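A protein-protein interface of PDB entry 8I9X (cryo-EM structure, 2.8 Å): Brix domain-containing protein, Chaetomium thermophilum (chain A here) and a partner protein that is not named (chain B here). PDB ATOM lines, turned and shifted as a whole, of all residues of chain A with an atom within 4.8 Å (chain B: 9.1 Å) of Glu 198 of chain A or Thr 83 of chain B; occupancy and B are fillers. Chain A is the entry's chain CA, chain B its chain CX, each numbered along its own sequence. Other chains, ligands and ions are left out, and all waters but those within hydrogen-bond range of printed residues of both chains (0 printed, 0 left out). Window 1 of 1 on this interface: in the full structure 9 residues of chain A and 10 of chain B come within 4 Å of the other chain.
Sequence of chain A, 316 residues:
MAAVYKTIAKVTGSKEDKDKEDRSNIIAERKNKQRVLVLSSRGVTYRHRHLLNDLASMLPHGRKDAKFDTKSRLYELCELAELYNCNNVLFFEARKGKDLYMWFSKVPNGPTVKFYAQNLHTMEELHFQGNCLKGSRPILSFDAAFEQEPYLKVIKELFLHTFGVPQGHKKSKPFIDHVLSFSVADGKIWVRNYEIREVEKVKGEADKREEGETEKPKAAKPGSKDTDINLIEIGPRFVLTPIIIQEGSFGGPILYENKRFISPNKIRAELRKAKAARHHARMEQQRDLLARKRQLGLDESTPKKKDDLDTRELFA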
ATOM      1  N   ILE A 196      -2.157   8.772  22.870  1.00  0.00           N
ATOM      2  CA  ILE A 196      -1.660  10.051  22.380  1.00  0.00           C
ATOM      3  C   ILE A 196      -0.622   9.740  21.306  1.00  0.00           C
ATOM      4  O   ILE A 196       0.495   9.323  21.611  1.00  0.00           O
ATOM      5  CB  ILE A 196      -1.066  10.892  23.512  1.00  0.00           C
ATOM      6  CG1 ILE A 196      -2.140  11.232  24.546  1.00  0.00           C
ATOM      7  CG2 ILE A 196      -0.403  12.144  22.968  1.00  0.00           C
ATOM      8  CD1 ILE A 196      -1.589  11.786  25.836  1.00  0.00           C
ATOM      9  N   ARG A 197      -0.989   9.925  20.044  1.00  0.00           N
ATOM     10  CA  ARG A 197      -0.092   9.685  18.925  1.00  0.00           C
ATOM     11  C   ARG A 197       0.453  11.016  18.432  1.00  0.00           C
ATOM     12  O   ARG A 197      -0.311  11.886  18.000  1.00  0.00           O
ATOM     13  CB  ARG A 197      -0.818   8.951  17.797  1.00  0.00           C
ATOM     14  CG  ARG A 197      -0.026   8.839  16.513  1.00  0.00           C
ATOM     15  CD  ARG A 197       0.957   7.690  16.586  1.00  0.00           C
ATOM     16  NE  ARG A 197       0.330   6.471  17.079  1.00  0.00           N
ATOM     17  CZ  ARG A 197      -0.383   5.640  16.331  1.00  0.00           C
ATOM     18  NH1 ARG A 197      -0.578   5.864  15.043  1.00  0.00           N
ATOM     19  NH2 ARG A 197      -0.910   4.555  16.890  1.00  0.00           N
ATOM     20  N   GLU A 198       1.767  11.179  18.505  1.00  0.00           N
ATOM     21  CA  GLU A 198       2.425  12.407  18.089  1.00  0.00           C
ATOM     22  C   GLU A 198       2.773  12.310  16.613  1.00  0.00           C
ATOM     23  O   GLU A 198       3.401  11.339  16.181  1.00  0.00           O
ATOM     24  CB  GLU A 198       3.682  12.658  18.921  1.00  0.00           C
ATOM     25  CG  GLU A 198       3.398  13.132  20.333  1.00  0.00           C
ATOM     26  CD  GLU A 198       4.654  13.250  21.170  1.00  0.00           C
ATOM     27  OE1 GLU A 198       5.594  12.459  20.949  1.00  0.00           O
ATOM     28  OE2 GLU A 198       4.701  14.134  22.051  1.00  0.00           O
ATOM     29  N   VAL A 199       2.357  13.310  15.840  1.00  0.00           N
ATOM     30  CA  VAL A 199       2.631  13.367  14.409  1.00  0.00           C
ATOM     31  C   VAL A 199       3.207  14.740  14.089  1.00  0.00           C
ATOM     32  O   VAL A 199       2.747  15.753  14.624  1.00  0.00           O
ATOM     33  CB  VAL A 199       1.374  13.068  13.570  1.00  0.00           C
ATOM     34  CG1 VAL A 199       0.883  11.661  13.841  1.00  0.00           C
ATOM     35  CG2 VAL A 199       0.268  14.048  13.874  1.00  0.00           C
ATOM     36  N   GLU A 200       4.230  14.762  13.238  1.00  0.00           N
ATOM     37  CA  GLU A 200       4.955  15.994  12.963  1.00  0.00           C
ATOM     38  C   GLU A 200       4.061  17.016  12.271  1.00  0.00           C
ATOM     39  O   GLU A 200       3.215  16.667  11.443  1.00  0.00           O
ATOM     40  CB  GLU A 200       6.182  15.701  12.100  1.00  0.00           C
ATOM     41  CG  GLU A 200       7.254  14.892  12.809  1.00  0.00           C
ATOM     42  CD  GLU A 200       8.444  14.593  11.919  1.00  0.00           C
ATOM     43  OE1 GLU A 200       8.382  14.912  10.713  1.00  0.00           O
ATOM     44  OE2 GLU A 200       9.442  14.039  12.427  1.00  0.00           O
ATOM     45  N   THR A 227       5.494  18.821  16.832  1.00  0.00           N
ATOM     46  CA  THR A 227       4.602  17.670  16.760  1.00  0.00           C
ATOM     47  C   THR A 227       3.276  17.962  17.447  1.00  0.00           C
ATOM     48  O   THR A 227       3.248  18.570  18.515  1.00  0.00           O
ATOM     49  CB  THR A 227       5.236  16.428  17.407  1.00  0.00           C
ATOM     50  OG1 THR A 227       5.363  16.635  18.818  1.00  0.00           O
ATOM     51  CG2 THR A 227       6.612  16.168  16.817  1.00  0.00           C
ATOM     52  N   ASP A 228       2.179  17.534  16.836  1.00  0.00           N
ATOM     53  CA  ASP A 228       0.862  17.678  17.435  1.00  0.00           C
ATOM     54  C   ASP A 228       0.224  16.315  17.688  1.00  0.00           C
ATOM     55  O   ASP A 228       0.699  15.276  17.222  1.00  0.00           O
ATOM     56  CB  ASP A 228      -0.045  18.560  16.568  1.00  0.00           C
ATOM     57  CG  ASP A 228      -0.117  18.104  15.127  1.00  0.00           C
ATOM     58  OD1 ASP A 228       0.134  16.917  14.856  1.00  0.00           O
ATOM     59  OD2 ASP A 228      -0.428  18.944  14.255  1.00  0.00           O
ATOM     60  N   PRO B  72      -3.170   2.244   8.891  1.00  0.00           N
ATOM     61  CA  PRO B  72      -2.518   3.005   9.963  1.00  0.00           C
ATOM     62  C   PRO B  72      -1.475   2.166  10.688  1.00  0.00           C
ATOM     63  O   PRO B  72      -1.585   0.941  10.780  1.00  0.00           O
ATOM     64  CB  PRO B  72      -3.682   3.371  10.890  1.00  0.00           C
ATOM     65  CG  PRO B  72      -4.883   3.345  10.014  1.00  0.00           C
ATOM     66  CD  PRO B  72      -4.634   2.234   9.033  1.00  0.00           C
ATOM     67  N   GLN B  73      -0.451   2.840  11.199  1.00  0.00           N
ATOM     68  CA  GLN B  73       0.558   2.180  12.012  1.00  0.00           C
ATOM     69  C   GLN B  73       0.010   1.902  13.405  1.00  0.00           C
ATOM     70  O   GLN B  73      -0.723   2.716  13.974  1.00  0.00           O
ATOM     71  CB  GLN B  73       1.822   3.035  12.100  1.00  0.00           C
ATOM     72  CG  GLN B  73       2.276   3.599  10.767  1.00  0.00           C
ATOM     73  CD  GLN B  73       3.540   4.421  10.886  1.00  0.00           C
ATOM     74  OE1 GLN B  73       4.513   3.997  11.509  1.00  0.00           O
ATOM     75  NE2 GLN B  73       3.535   5.604  10.284  1.00  0.00           N
ATOM     76  N   LEU B  74       0.371   0.746  13.953  1.00  0.00           N
ATOM     77  CA  LEU B  74      -0.171   0.269  15.216  1.00  0.00           C
ATOM     78  C   LEU B  74       0.933   0.201  16.262  1.00  0.00           C
ATOM     79  O   LEU B  74       2.036  -0.278  15.983  1.00  0.00           O
ATOM     80  CB  LEU B  74      -0.812  -1.109  15.039  1.00  0.00           C
ATOM     81  CG  LEU B  74      -2.051  -1.142  14.146  1.00  0.00           C
ATOM     82  CD1 LEU B  74      -2.517  -2.570  13.930  1.00  0.00           C
ATOM     83  CD2 LEU B  74      -3.163  -0.293  14.736  1.00  0.00           C
ATOM     84  N   ASN B  75       0.627   0.669  17.469  1.00  0.00           N
ATOM     85  CA  ASN B  75       1.609   0.752  18.543  1.00  0.00           C
ATOM     86  C   ASN B  75       1.695  -0.591  19.256  1.00  0.00           C
ATOM     87  O   ASN B  75       0.694  -1.090  19.780  1.00  0.00           O
ATOM     88  CB  ASN B  75       1.245   1.867  19.522  1.00  0.00           C
ATOM     89  CG  ASN B  75       2.366   2.185  20.487  1.00  0.00           C
ATOM     90  OD1 ASN B  75       3.538   1.956  20.190  1.00  0.00           O
ATOM     91  ND2 ASN B  75       2.014   2.726  21.646  1.00  0.00           N
ATOM     92  N   PRO B  79       7.854   0.484  19.289  1.00  0.00           N
ATOM     93  CA  PRO B  79       7.137   1.765  19.251  1.00  0.00           C
ATOM     94  C   PRO B  79       6.926   2.263  17.829  1.00  0.00           C
ATOM     95  O   PRO B  79       7.769   2.071  16.950  1.00  0.00           O
ATOM     96  CB  PRO B  79       8.056   2.703  20.041  1.00  0.00           C
ATOM     97  CG  PRO B  79       8.904   1.807  20.870  1.00  0.00           C
ATOM     98  CD  PRO B  79       9.110   0.579  20.049  1.00  0.00           C
ATOM     99  N   VAL B  80       5.781   2.909  17.605  1.00  0.00           N
ATOM    100  CA  VAL B  80       5.549   3.600  16.339  1.00  0.00           C
ATOM    101  C   VAL B  80       6.391   4.867  16.264  1.00  0.00           C
ATOM    102  O   VAL B  80       6.869   5.256  15.192  1.00  0.00           O
ATOM    103  CB  VAL B  80       4.053   3.902  16.148  1.00  0.00           C
ATOM    104  CG1 VAL B  80       3.286   2.623  15.954  1.00  0.00           C
ATOM    105  CG2 VAL B  80       3.503   4.660  17.345  1.00  0.00           C
ATOM    106  N   GLY B  81       6.578   5.531  17.395  1.00  0.00           N
ATOM    107  CA  GLY B  81       7.289   6.786  17.412  1.00  0.00           C
ATOM    108  C   GLY B  81       6.432   7.924  16.901  1.00  0.00           C
ATOM    109  O   GLY B  81       5.206   7.834  16.785  1.00  0.00           O
ATOM    110  N   VAL B  82       7.106   9.025  16.588  1.00  0.00           N
ATOM    111  CA  VAL B  82       6.439  10.199  16.035  1.00  0.00           C
ATOM    112  C   VAL B  82       6.294   9.986  14.532  1.00  0.00           C
ATOM    113  O   VAL B  82       7.250  10.164  13.775  1.00  0.00           O
ATOM    114  CB  VAL B  82       7.212  11.484  16.345  1.00  0.00           C
ATOM    115  CG1 VAL B  82       6.550  12.671  15.669  1.00  0.00           C
ATOM    116  CG2 VAL B  82       7.301  11.697  17.844  1.00  0.00           C
ATOM    117  N   THR B  83       5.099   9.598  14.101  1.00  0.00           N
ATOM    118  CA  THR B  83       4.867   9.307  12.696  1.00  0.00           C
ATOM    119  C   THR B  83       4.741  10.596  11.895  1.00  0.00           C
ATOM    120  O   THR B  83       4.465  11.669  12.436  1.00  0.00           O
ATOM    121  CB  THR B  83       3.611   8.455  12.518  1.00  0.00           C
ATOM    122  OG1 THR B  83       2.453   9.295  12.552  1.00  0.00           O
ATOM    123  CG2 THR B  83       3.511   7.419  13.625  1.00  0.00           C
ATOM    124  N   LYS B  84       4.952  10.480  10.590  1.00  0.00           N
ATOM    125  CA  LYS B  84       4.963  11.621   9.689  1.00  0.00           C
ATOM    126  C   LYS B  84       3.661  11.703   8.905  1.00  0.00           C
ATOM    127  O   LYS B  84       3.120  10.670   8.493  1.00  0.00           O
ATOM    128  CB  LYS B  84       6.139  11.515   8.719  1.00  0.00           C
ATOM    129  CG  LYS B  84       7.455  11.184   9.402  1.00  0.00           C
ATOM    130  CD  LYS B  84       8.594  11.097   8.405  1.00  0.00           C
ATOM    131  CE  LYS B  84       9.850  11.742   8.958  1.00  0.00           C
ATOM    132  NZ  LYS B  84      10.191  11.214  10.306  1.00  0.00           N
ATOM    133  N   PRO B  85       3.135  12.906   8.686  1.00  0.00           N
ATOM    134  CA  PRO B  85       1.859  13.027   7.972  1.00  0.00           C
ATOM    135  C   PRO B  85       1.986  12.575   6.526  1.00  0.00           C
ATOM    136  O   PRO B  85       3.035  12.719   5.895  1.00  0.00           O
ATOM    137  CB  PRO B  85       1.524  14.521   8.072  1.00  0.00           C
ATOM    138  CG  PRO B  85       2.763  15.204   8.523  1.00  0.00           C
ATOM    139  CD  PRO B  85       3.808  14.201   8.876  1.00  0.00           C
ATOM    140  N   LYS B  86       0.897  12.024   6.006  1.00  0.00           N
ATOM    141  CA  LYS B  86       0.893  11.414   4.686  1.00  0.00           C
ATOM    142  C   LYS B  86       0.872  12.480   3.596  1.00  0.00           C
ATOM    143  O   LYS B  86       0.203  13.510   3.717  1.00  0.00           O
ATOM    144  CB  LYS B  86      -0.310  10.482   4.529  1.00  0.00           C
ATOM    145  CG  LYS B  86      -0.399   9.792   3.180  1.00  0.00           C
ATOM    146  CD  LYS B  86       0.736   8.800   2.993  1.00  0.00           C
ATOM    147  CE  LYS B  86       0.563   7.997   1.714  1.00  0.00           C
ATOM    148  NZ  LYS B  86       0.686   8.851   0.500  1.00  0.00           N
ATOM    149  N   LYS B  89       6.192  16.412   3.422  1.00  0.00           N
ATOM    150  CA  LYS B  89       7.645  16.333   3.354  1.00  0.00           C
ATOM    151  C   LYS B  89       8.224  15.463   4.461  1.00  0.00           C
ATOM    152  O   LYS B  89       8.346  15.904   5.608  1.00  0.00           O
ATOM    153  CB  LYS B  89       8.251  17.736   3.421  1.00  0.00           C
ATOM    154  CG  LYS B  89       9.765  17.762   3.334  1.00  0.00           C
ATOM    155  CD  LYS B  89      10.340  18.994   4.010  1.00  0.00           C
ATOM    156  CE  LYS B  89      11.856  19.010   3.924  1.00  0.00           C
ATOM    157  NZ  LYS B  89      12.342  19.775   2.745  1.00  0.00           N
ATOM    158  N   LYS B  90       8.587  14.226   4.124  1.00  0.00           N
ATOM    159  CA  LYS B  90       9.308  13.363   5.050  1.00  0.00           C
ATOM    160  C   LYS B  90      10.775  13.767   5.069  1.00  0.00           C
ATOM    161  O   LYS B  90      11.517  13.445   4.136  1.00  0.00           O
ATOM    162  CB  LYS B  90       9.169  11.894   4.651  1.00  0.00           C
ATOM    163  CG  LYS B  90       7.752  11.360   4.694  1.00  0.00           C
ATOM    164  CD  LYS B  90       7.734   9.852   4.506  1.00  0.00           C
ATOM    165  CE  LYS B  90       8.055   9.469   3.071  1.00  0.00           C
ATOM    166  NZ  LYS B  90       7.916   8.005   2.846  1.00  0.00           N
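Val 80 of chain B touches Arg 197 of chain A (CG2 to NE, 3.7 Å). Arg 197 of chain A touches Thr 83 of chain B. Glu 198 of chain A touches Gly 81 of chain B. Val 82 of chain B touches Glu 198 of chain A (CA to O, 3.2 Å). Thr 83 of chain B touches Val 199 of chain A. Glu 200 of chain A touches Val 82 of chain B. Glu 200 of chain A touches Pro 85 of chain B (O to CG, 3.3 Å). Thr 227 of chain A touches Val 82 of chain B.
N of Thr 83 of chain B sits at hydrogen-bond distance from O of Glu 198 of chain A (3.2 Å). NH1 of Arg 197 of chain A lies within hydrogen-bond range of O of Gln 73 of chain B (3.3 Å). The side-chain amino group of Lys 84 of chain B is in salt-bridge range of the side-chain carboxylate of Glu 200 of chain A, 3.6 Å away. The backbone carbonyl oxygen (O) of Thr 83 of chain B lies within hydrogen-bond range of the backbone NH (N) of Glu 200 of chain A, 3.2 Å away.
Hydrophobic or aromatic side chains of chain B within 4 Å of the printed part of chain A: Val 80, Val 82 and Pro 85. Printed residues of chain A that touch a printed residue of chain B: Arg 197, Glu 198, Val 199, Glu 200 and Thr 227. Hydrophobic or aromatic side chains of chain A within 4 Å of the printed part of chain B: Val 199. Among the printed residues, Asp or Glu carboxylates within 4 Å of a Lys or Arg side-chain nitrogen of the other chain: Glu 200 of chain A with Lys 84 of chain B (3.6 Å).
O of Val 199 of chain A lies within hydrogen-bond range of N of Asp 228 of chain A (2.9 Å).
Of the printed residues of chain B, Glu 198 of chain A touches Gly 81 (3.99 Å), Val 82 (3.2 Å) and Thr 83 (3.2 Å). Of chain B, only Thr 83 comes within 4 Å of Val 199 of chain A. Printed residues of chain B within 4 Å of Glu 200 of chain A: Val 82, Thr 83, Lys 84 and Pro 85. Pro 72 of chain B touches none of the printed residues of chain A. Of the printed residues of chain A, Gln 73 of chain B touches Arg 197. Pro 79 of chain B touches none of the printed residues of chain A. Of the printed residues of chain A, Val 82 of chain B touches Glu 198, Glu 200 and Thr 227. Of chain A, only Arg 197 (3.9 Å), Glu 198 (3.2 Å), Val 199 (3.1 Å) and Glu 200 (3.2 Å) come within 4 Å of Thr 83 of chain B. The nearest printed residue of chain B that does not touch Thr 227 of chain A is Thr 83 of chain B (6.6 Å).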
